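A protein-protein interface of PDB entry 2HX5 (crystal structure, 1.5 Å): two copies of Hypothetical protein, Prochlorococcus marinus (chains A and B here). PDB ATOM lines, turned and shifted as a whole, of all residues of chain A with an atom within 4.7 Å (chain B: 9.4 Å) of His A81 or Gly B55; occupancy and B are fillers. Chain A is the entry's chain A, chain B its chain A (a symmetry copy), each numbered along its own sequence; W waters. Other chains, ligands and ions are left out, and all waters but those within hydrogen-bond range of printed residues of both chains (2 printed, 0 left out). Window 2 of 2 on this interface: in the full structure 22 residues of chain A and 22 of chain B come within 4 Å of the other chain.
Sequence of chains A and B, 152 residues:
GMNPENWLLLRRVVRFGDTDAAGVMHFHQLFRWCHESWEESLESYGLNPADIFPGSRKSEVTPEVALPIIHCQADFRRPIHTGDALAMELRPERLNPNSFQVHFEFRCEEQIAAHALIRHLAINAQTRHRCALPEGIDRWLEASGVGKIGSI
The backbone carbonyl oxygen of Pro A79 is in hydrogen-bond range of the guanidinium group of Arg B57, at 3.1 Å. The backbone carbonyl oxygen (O) of Gly B55 lies close to the backbone NH (N) of Thr A82, at 3.3 Å. OD2 of Asp A84 lies within salt-bridge range of NH2 of Arg B57 (2.6 Å). The backbone carbonyl oxygen (O) of Gly B55 lies close to the backbone carbonyl oxygen (O) of Gly A23. The backbone carbonyl oxygen of Thr A82 is in hydrogen-bond range of the side-chain hydroxyl of Ser B56, 3.5 Å away.
The backbone NH (N) of Val A14 is in hydrogen-bond range of the backbone carbonyl oxygen (O) of Asp A84, at 2.9 Å. O of Pro B49 is in hydrogen-bond range of OG of Ser B56 (3.3 Å). O of Phe B53 sits at hydrogen-bond distance from OG of Ser B56 (2.9 Å). N of His A81 is in hydrogen-bond range of OD2 of Asp A84 (2.8 Å).
Gly B55 touches His A81. CB of His A81 touches N of Arg B57, 3.6 Å away. Thr A82 touches Pro B54 (CG2 to O, 2.9 Å).
No residue of chain B comes within 4 Å of Val A14. Of the printed residues of chain B, Gly A23 touches Gly B55 (3.4 Å). Of the printed residues of chain B, Pro A79 touches Arg B57 (3.1 Å). His A81 touches just these residues of chain B: Gly B55 (3.0 Å) and Arg B57 (3.6 Å). Printed residues of chain B within 4 Å of Thr A82: Pro B54, Gly B55 and Ser B56. Gly A83 touches none of the printed residues of chain B. Asp A84 touches just one residue of chain B: Arg B57 (2.6 Å). Printed residues of chain A within 4 Å of Gly B55: Gly A23 (3.4 Å), His A81 (3.0 Å) and Thr A82 (3.2 Å). The nearest residue of chain B that does not touch His A81 is Ser B56 (4.1 Å). The nearest printed residue of chain A that does not touch Gly B55 is Val A24 (5.3 Å).
Of the 15 printed residues of chain B, 4 touch a printed residue of chain A. Of the 9 printed residues of chain A, 5 touch a printed residue of chain B. Printed residues of chain A that touch a printed residue of chain B: Gly A23, Pro A79, His A81, Thr A82 and Asp A84. Among the printed residues, 8 pairs touch across the chains. Among the printed residues, Asp or Glu carboxylates within 4 Å of a Lys or Arg side-chain nitrogen of the other chain: Asp A84 with Arg B57 (2.6 Å).
No position is printed for both chains.
Water W2 lies within hydrogen-bond range of O of Pro A79 (2.8 Å) and NH1 of Arg B57 (2.9 Å). Water W1 lies within hydrogen-bond range of O of Thr A82, N of Arg B57 and OD1 of Asp A84.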
ATOM      1  N   VAL A  14      25.893 -20.249  24.176  1.00  0.00           N
ATOM      2  CA  VAL A  14      25.913 -20.729  22.802  1.00  0.00           C
ATOM      3  C   VAL A  14      24.963 -21.963  22.702  1.00  0.00           C
ATOM      4  O   VAL A  14      25.053 -22.875  23.500  1.00  0.00           O
ATOM      5  CB  VAL A  14      27.347 -21.118  22.341  1.00  0.00           C
ATOM      6  CG1 VAL A  14      27.336 -21.583  20.902  1.00  0.00           C
ATOM      7  CG2 VAL A  14      28.336 -19.931  22.566  1.00  0.00           C
ATOM      8  N   GLY A  23      31.658 -28.340  14.075  1.00  0.00           N
ATOM      9  CA  GLY A  23      31.588 -28.568  15.526  1.00  0.00           C
ATOM     10  C   GLY A  23      31.778 -27.307  16.353  1.00  0.00           C
ATOM     11  O   GLY A  23      32.066 -27.402  17.551  1.00  0.00           O
ATOM     12  N   VAL A  24      31.615 -26.120  15.749  1.00  0.00           N
ATOM     13  CA  VAL A  24      31.851 -24.825  16.371  1.00  0.00           C
ATOM     14  C   VAL A  24      30.835 -23.799  15.833  1.00  0.00           C
ATOM     15  O   VAL A  24      30.130 -24.081  14.866  1.00  0.00           O
ATOM     16  CB  VAL A  24      33.257 -24.286  16.082  1.00  0.00           C
ATOM     17  CG1 VAL A  24      34.328 -25.131  16.822  1.00  0.00           C
ATOM     18  CG2 VAL A  24      33.486 -24.219  14.616  1.00  0.00           C
ATOM     19  N   PRO A  79      37.978 -20.823  18.951  1.00  0.00           N
ATOM     20  CA  PRO A  79      36.716 -21.500  18.647  1.00  0.00           C
ATOM     21  C   PRO A  79      35.686 -21.376  19.775  1.00  0.00           C
ATOM     22  O   PRO A  79      36.026 -21.385  20.972  1.00  0.00           O
ATOM     23  CB  PRO A  79      37.114 -22.962  18.454  1.00  0.00           C
ATOM     24  CG  PRO A  79      38.457 -23.076  18.977  1.00  0.00           C
ATOM     25  CD  PRO A  79      39.116 -21.743  18.983  1.00  0.00           C
ATOM     26  N   ILE A  80      34.419 -21.294  19.366  1.00  0.00           N
ATOM     27  CA  ILE A  80      33.310 -21.116  20.273  1.00  0.00           C
ATOM     28  C   ILE A  80      32.404 -22.301  20.089  1.00  0.00           C
ATOM     29  O   ILE A  80      32.110 -22.680  18.939  1.00  0.00           O
ATOM     30  CB  ILE A  80      32.550 -19.789  19.949  1.00  0.00           C
ATOM     31  CG1 ILE A  80      33.442 -18.581  20.309  1.00  0.00           C
ATOM     32  CG2 ILE A  80      31.144 -19.685  20.685  1.00  0.00           C
ATOM     33  CD1 ILE A  80      32.949 -17.225  19.781  1.00  0.00           C
ATOM     34  N   HIS A  81      32.006 -22.916  21.194  1.00  0.00           N
ATOM     35  CA  HIS A  81      31.313 -24.215  21.207  1.00  0.00           C
ATOM     36  C   HIS A  81      29.932 -24.207  21.817  1.00  0.00           C
ATOM     37  O   HIS A  81      29.633 -23.381  22.654  1.00  0.00           O
ATOM     38  CB  HIS A  81      32.163 -25.209  22.032  1.00  0.00           C
ATOM     39  CG  HIS A  81      33.400 -25.631  21.334  1.00  0.00           C
ATOM     40  ND1 HIS A  81      34.652 -25.162  21.679  1.00  0.00           N
ATOM     41  CD2 HIS A  81      33.581 -26.473  20.291  1.00  0.00           C
ATOM     42  CE1 HIS A  81      35.551 -25.695  20.867  1.00  0.00           C
ATOM     43  NE2 HIS A  81      34.927 -26.468  19.997  1.00  0.00           N
ATOM     44  N   THR A  82      29.088 -25.160  21.418  1.00  0.00           N
ATOM     45  CA  THR A  82      27.764 -25.282  22.014  1.00  0.00           C
ATOM     46  C   THR A  82      27.867 -25.430  23.550  1.00  0.00           C
ATOM     47  O   THR A  82      28.653 -26.235  24.081  1.00  0.00           O
ATOM     48  CB  THR A  82      26.856 -26.384  21.312  1.00  0.00           C
ATOM     49  OG1 THR A  82      25.919 -26.924  22.244  1.00  0.00           O
ATOM     50  CG2 THR A  82      27.671 -27.532  20.763  1.00  0.00           C
ATOM     51  N   GLY A  83      27.068 -24.647  24.255  1.00  0.00           N
ATOM     52  CA  GLY A  83      27.038 -24.658  25.686  1.00  0.00           C
ATOM     53  C   GLY A  83      28.046 -23.721  26.320  1.00  0.00           C
ATOM     54  O   GLY A  83      27.986 -23.583  27.534  1.00  0.00           O
ATOM     55  N   ASP A  84      28.955 -23.094  25.557  1.00  0.00           N
ATOM     56  CA  ASP A  84      29.859 -22.061  26.100  1.00  0.00           C
ATOM     57  C   ASP A  84      29.053 -20.915  26.693  1.00  0.00           C
ATOM     58  O   ASP A  84      28.086 -20.464  26.084  1.00  0.00           O
ATOM     59  CB  ASP A  84      30.813 -21.502  25.069  1.00  0.00           C
ATOM     60  CG  ASP A  84      32.011 -22.403  24.754  1.00  0.00           C
ATOM     61  OD1 ASP A  84      32.298 -23.386  25.477  1.00  0.00           O
ATOM     62  OD2 ASP A  84      32.691 -22.112  23.749  1.00  0.00           O
ATOM     63  N   GLU B  39      17.018 -26.725  25.358  1.00  0.00           N
ATOM     64  CA  GLU B  39      18.401 -26.732  25.848  1.00  0.00           C
ATOM     65  C   GLU B  39      18.489 -26.018  27.197  1.00  0.00           C
ATOM     66  O   GLU B  39      19.167 -26.475  28.115  1.00  0.00           O
ATOM     67  CB  GLU B  39      19.321 -26.050  24.824  1.00  0.00           C
ATOM     68  CG  GLU B  39      19.378 -26.749  23.488  1.00  0.00           C
ATOM     69  CD  GLU B  39      20.141 -25.945  22.443  1.00  0.00           C
ATOM     70  OE1 GLU B  39      21.391 -25.840  22.580  1.00  0.00           O
ATOM     71  OE2 GLU B  39      19.459 -25.438  21.522  1.00  0.00           O
ATOM     72  N   PRO B  49      25.846 -29.890  29.017  1.00  0.00           N
ATOM     73  CA  PRO B  49      25.770 -29.954  27.545  1.00  0.00           C
ATOM     74  C   PRO B  49      26.710 -30.984  26.937  1.00  0.00           C
ATOM     75  O   PRO B  49      26.356 -31.602  25.930  1.00  0.00           O
ATOM     76  CB  PRO B  49      26.244 -28.539  27.077  1.00  0.00           C
ATOM     77  CG  PRO B  49      26.757 -27.845  28.271  1.00  0.00           C
ATOM     78  CD  PRO B  49      26.041 -28.490  29.461  1.00  0.00           C
ATOM     79  N   ALA B  50      27.890 -31.091  27.528  1.00  0.00           N
ATOM     80  CA  ALA B  50      28.941 -31.996  27.106  1.00  0.00           C
ATOM     81  C   ALA B  50      28.513 -33.469  27.053  1.00  0.00           C
ATOM     82  O   ALA B  50      29.118 -34.255  26.297  1.00  0.00           O
ATOM     83  CB  ALA B  50      30.207 -31.810  27.986  1.00  0.00           C
ATOM     84  N   ASP B  51      27.515 -33.841  27.861  1.00  0.00           N
ATOM     85  CA  ASP B  51      26.975 -35.191  27.854  1.00  0.00           C
ATOM     86  C   ASP B  51      25.893 -35.457  26.833  1.00  0.00           C
ATOM     87  O   ASP B  51      25.556 -36.609  26.543  1.00  0.00           O
ATOM     88  CB  ASP B  51      26.394 -35.493  29.238  1.00  0.00           C
ATOM     89  CG  ASP B  51      27.448 -35.494  30.339  1.00  0.00           C
ATOM     90  OD1 ASP B  51      28.649 -35.824  30.068  1.00  0.00           O
ATOM     91  OD2 ASP B  51      27.080 -35.154  31.484  1.00  0.00           O
ATOM     92  N   ILE B  52      25.312 -34.400  26.279  1.00  0.00           N
ATOM     93  CA  ILE B  52      24.147 -34.557  25.385  1.00  0.00           C
ATOM     94  C   ILE B  52      24.378 -34.072  23.960  1.00  0.00           C
ATOM     95  O   ILE B  52      23.958 -34.736  23.009  1.00  0.00           O
ATOM     96  CB  ILE B  52      22.846 -33.892  25.982  1.00  0.00           C
ATOM     97  CG1 ILE B  52      22.595 -34.408  27.413  1.00  0.00           C
ATOM     98  CG2 ILE B  52      21.610 -34.107  25.029  1.00  0.00           C
ATOM     99  CD1 ILE B  52      21.508 -33.685  28.191  1.00  0.00           C
ATOM    100  N   PHE B  53      25.032 -32.923  23.805  1.00  0.00           N
ATOM    101  CA  PHE B  53      25.109 -32.253  22.496  1.00  0.00           C
ATOM    102  C   PHE B  53      26.501 -32.368  21.920  1.00  0.00           C
ATOM    103  O   PHE B  53      27.470 -32.031  22.566  1.00  0.00           O
ATOM    104  CB  PHE B  53      24.712 -30.752  22.600  1.00  0.00           C
ATOM    105  CG  PHE B  53      23.257 -30.556  22.944  1.00  0.00           C
ATOM    106  CD1 PHE B  53      22.259 -30.654  21.979  1.00  0.00           C
ATOM    107  CD2 PHE B  53      22.883 -30.338  24.268  1.00  0.00           C
ATOM    108  CE1 PHE B  53      20.903 -30.503  22.330  1.00  0.00           C
ATOM    109  CE2 PHE B  53      21.528 -30.168  24.600  1.00  0.00           C
ATOM    110  CZ  PHE B  53      20.560 -30.282  23.649  1.00  0.00           C
ATOM    111  N   PRO B  54      26.591 -32.814  20.650  1.00  0.00           N
ATOM    112  CA  PRO B  54      27.893 -32.732  20.012  1.00  0.00           C
ATOM    113  C   PRO B  54      28.298 -31.245  19.856  1.00  0.00           C
ATOM    114  O   PRO B  54      27.453 -30.313  19.910  1.00  0.00           O
ATOM    115  CB  PRO B  54      27.661 -33.389  18.645  1.00  0.00           C
ATOM    116  CG  PRO B  54      26.300 -33.720  18.534  1.00  0.00           C
ATOM    117  CD  PRO B  54      25.549 -33.375  19.771  1.00  0.00           C
ATOM    118  N   GLY B  55      29.592 -31.054  19.649  1.00  0.00           N
ATOM    119  CA  GLY B  55      30.155 -29.716  19.463  1.00  0.00           C
ATOM    120  C   GLY B  55      30.514 -29.000  20.761  1.00  0.00           C
ATOM    121  O   GLY B  55      30.882 -27.814  20.733  1.00  0.00           O
ATOM    122  N   SER B  56      30.399 -29.689  21.898  1.00  0.00           N
ATOM    123  CA  SER B  56      30.547 -29.030  23.185  1.00  0.00           C
ATOM    124  C   SER B  56      32.016 -29.003  23.534  1.00  0.00           C
ATOM    125  O   SER B  56      32.790 -29.839  23.093  1.00  0.00           O
ATOM    126  CB  SER B  56      29.740 -29.756  24.273  1.00  0.00           C
ATOM    127  OG  SER B  56      28.317 -29.704  24.059  1.00  0.00           O
ATOM    128  N   ARG B  57      32.430 -28.016  24.315  1.00  0.00           N
ATOM    129  CA  ARG B  57      33.841 -27.816  24.574  1.00  0.00           C
ATOM    130  C   ARG B  57      34.428 -28.962  25.417  1.00  0.00           C
ATOM    131  O   ARG B  57      35.524 -29.383  25.153  1.00  0.00           O
ATOM    132  CB  ARG B  57      34.071 -26.494  25.330  1.00  0.00           C
ATOM    133  CG  ARG B  57      35.509 -26.219  25.719  1.00  0.00           C
ATOM    134  CD  ARG B  57      35.628 -24.848  26.423  1.00  0.00           C
ATOM    135  NE  ARG B  57      35.148 -23.733  25.577  1.00  0.00           N
ATOM    136  CZ  ARG B  57      35.829 -23.213  24.556  1.00  0.00           C
ATOM    137  NH1 ARG B  57      37.028 -23.676  24.231  1.00  0.00           N
ATOM    138  NH2 ARG B  57      35.317 -22.207  23.849  1.00  0.00           N
ATOM    139  N   LYS B  58      33.674 -29.463  26.404  1.00  0.00           N
ATOM    140  CA  LYS B  58      34.269 -30.292  27.474  1.00  0.00           C
ATOM    141  C   LYS B  58      33.928 -31.782  27.372  1.00  0.00           C
ATOM    142  O   LYS B  58      34.199 -32.535  28.316  1.00  0.00           O
ATOM    143  CB  LYS B  58      33.862 -29.727  28.851  1.00  0.00           C
ATOM    144  CG  LYS B  58      34.423 -28.299  29.102  1.00  0.00           C
ATOM    145  CD  LYS B  58      34.003 -27.774  30.446  1.00  0.00           C
ATOM    146  CE  LYS B  58      34.505 -26.351  30.689  1.00  0.00           C
ATOM    147  NZ  LYS B  58      33.607 -25.679  31.701  1.00  0.00           N
ATOM    148  N   SER B  59      33.400 -32.213  26.230  1.00  0.00           N
ATOM    149  CA  SER B  59      33.094 -33.633  26.011  1.00  0.00           C
ATOM    150  C   SER B  59      34.378 -34.450  26.014  1.00  0.00           C
ATOM    151  O   SER B  59      35.391 -34.117  25.372  1.00  0.00           O
ATOM    152  CB  SER B  59      32.350 -33.859  24.707  1.00  0.00           C
ATOM    153  OG  SER B  59      31.080 -33.197  24.685  1.00  0.00           O
ATOM    154  N   VAL B  61      34.209 -37.651  25.098  1.00  0.00           N
ATOM    155  CA  VAL B  61      33.942 -38.249  23.797  1.00  0.00           C
ATOM    156  C   VAL B  61      32.665 -37.642  23.279  1.00  0.00           C
ATOM    157  O   VAL B  61      31.872 -37.083  24.025  1.00  0.00           O
ATOM    158  CB  VAL B  61      33.787 -39.785  23.830  1.00  0.00           C
ATOM    159  CG1 VAL B  61      35.139 -40.447  24.198  1.00  0.00           C
ATOM    160  CG2 VAL B  61      32.649 -40.192  24.793  1.00  0.00           C
ATOM    161  N   THR B  62      32.470 -37.704  21.977  1.00  0.00           N
ATOM    162  CA  THR B  62      31.239 -37.176  21.434  1.00  0.00           C
ATOM    163  C   THR B  62      30.079 -38.035  21.969  1.00  0.00           C
ATOM    164  O   THR B  62      30.192 -39.255  22.112  1.00  0.00           O
ATOM    165  CB  THR B  62      31.288 -37.039  19.892  1.00  0.00           C
ATOM    166  OG1 THR B  62      30.096 -36.362  19.414  1.00  0.00           O
ATOM    167  CG2 THR B  62      31.424 -38.368  19.253  1.00  0.00           C
ATOM    168  N   PRO B  63      28.981 -37.379  22.364  1.00  0.00           N
ATOM    169  CA  PRO B  63      27.880 -38.138  22.904  1.00  0.00           C
ATOM    170  C   PRO B  63      27.448 -39.293  21.967  1.00  0.00           C
ATOM    171  O   PRO B  63      27.363 -39.117  20.742  1.00  0.00           O
ATOM    172  CB  PRO B  63      26.789 -37.092  23.046  1.00  0.00           C
ATOM    173  CG  PRO B  63      27.543 -35.808  23.247  1.00  0.00           C
ATOM    174  CD  PRO B  63      28.734 -35.930  22.347  1.00  0.00           C
HETATM  175  O   HOH W   1      30.988 -25.936  25.550  1.00  0.00           O
HETATM  176  O   HOH W   2      38.373 -21.992  22.273  1.00  0.00           O
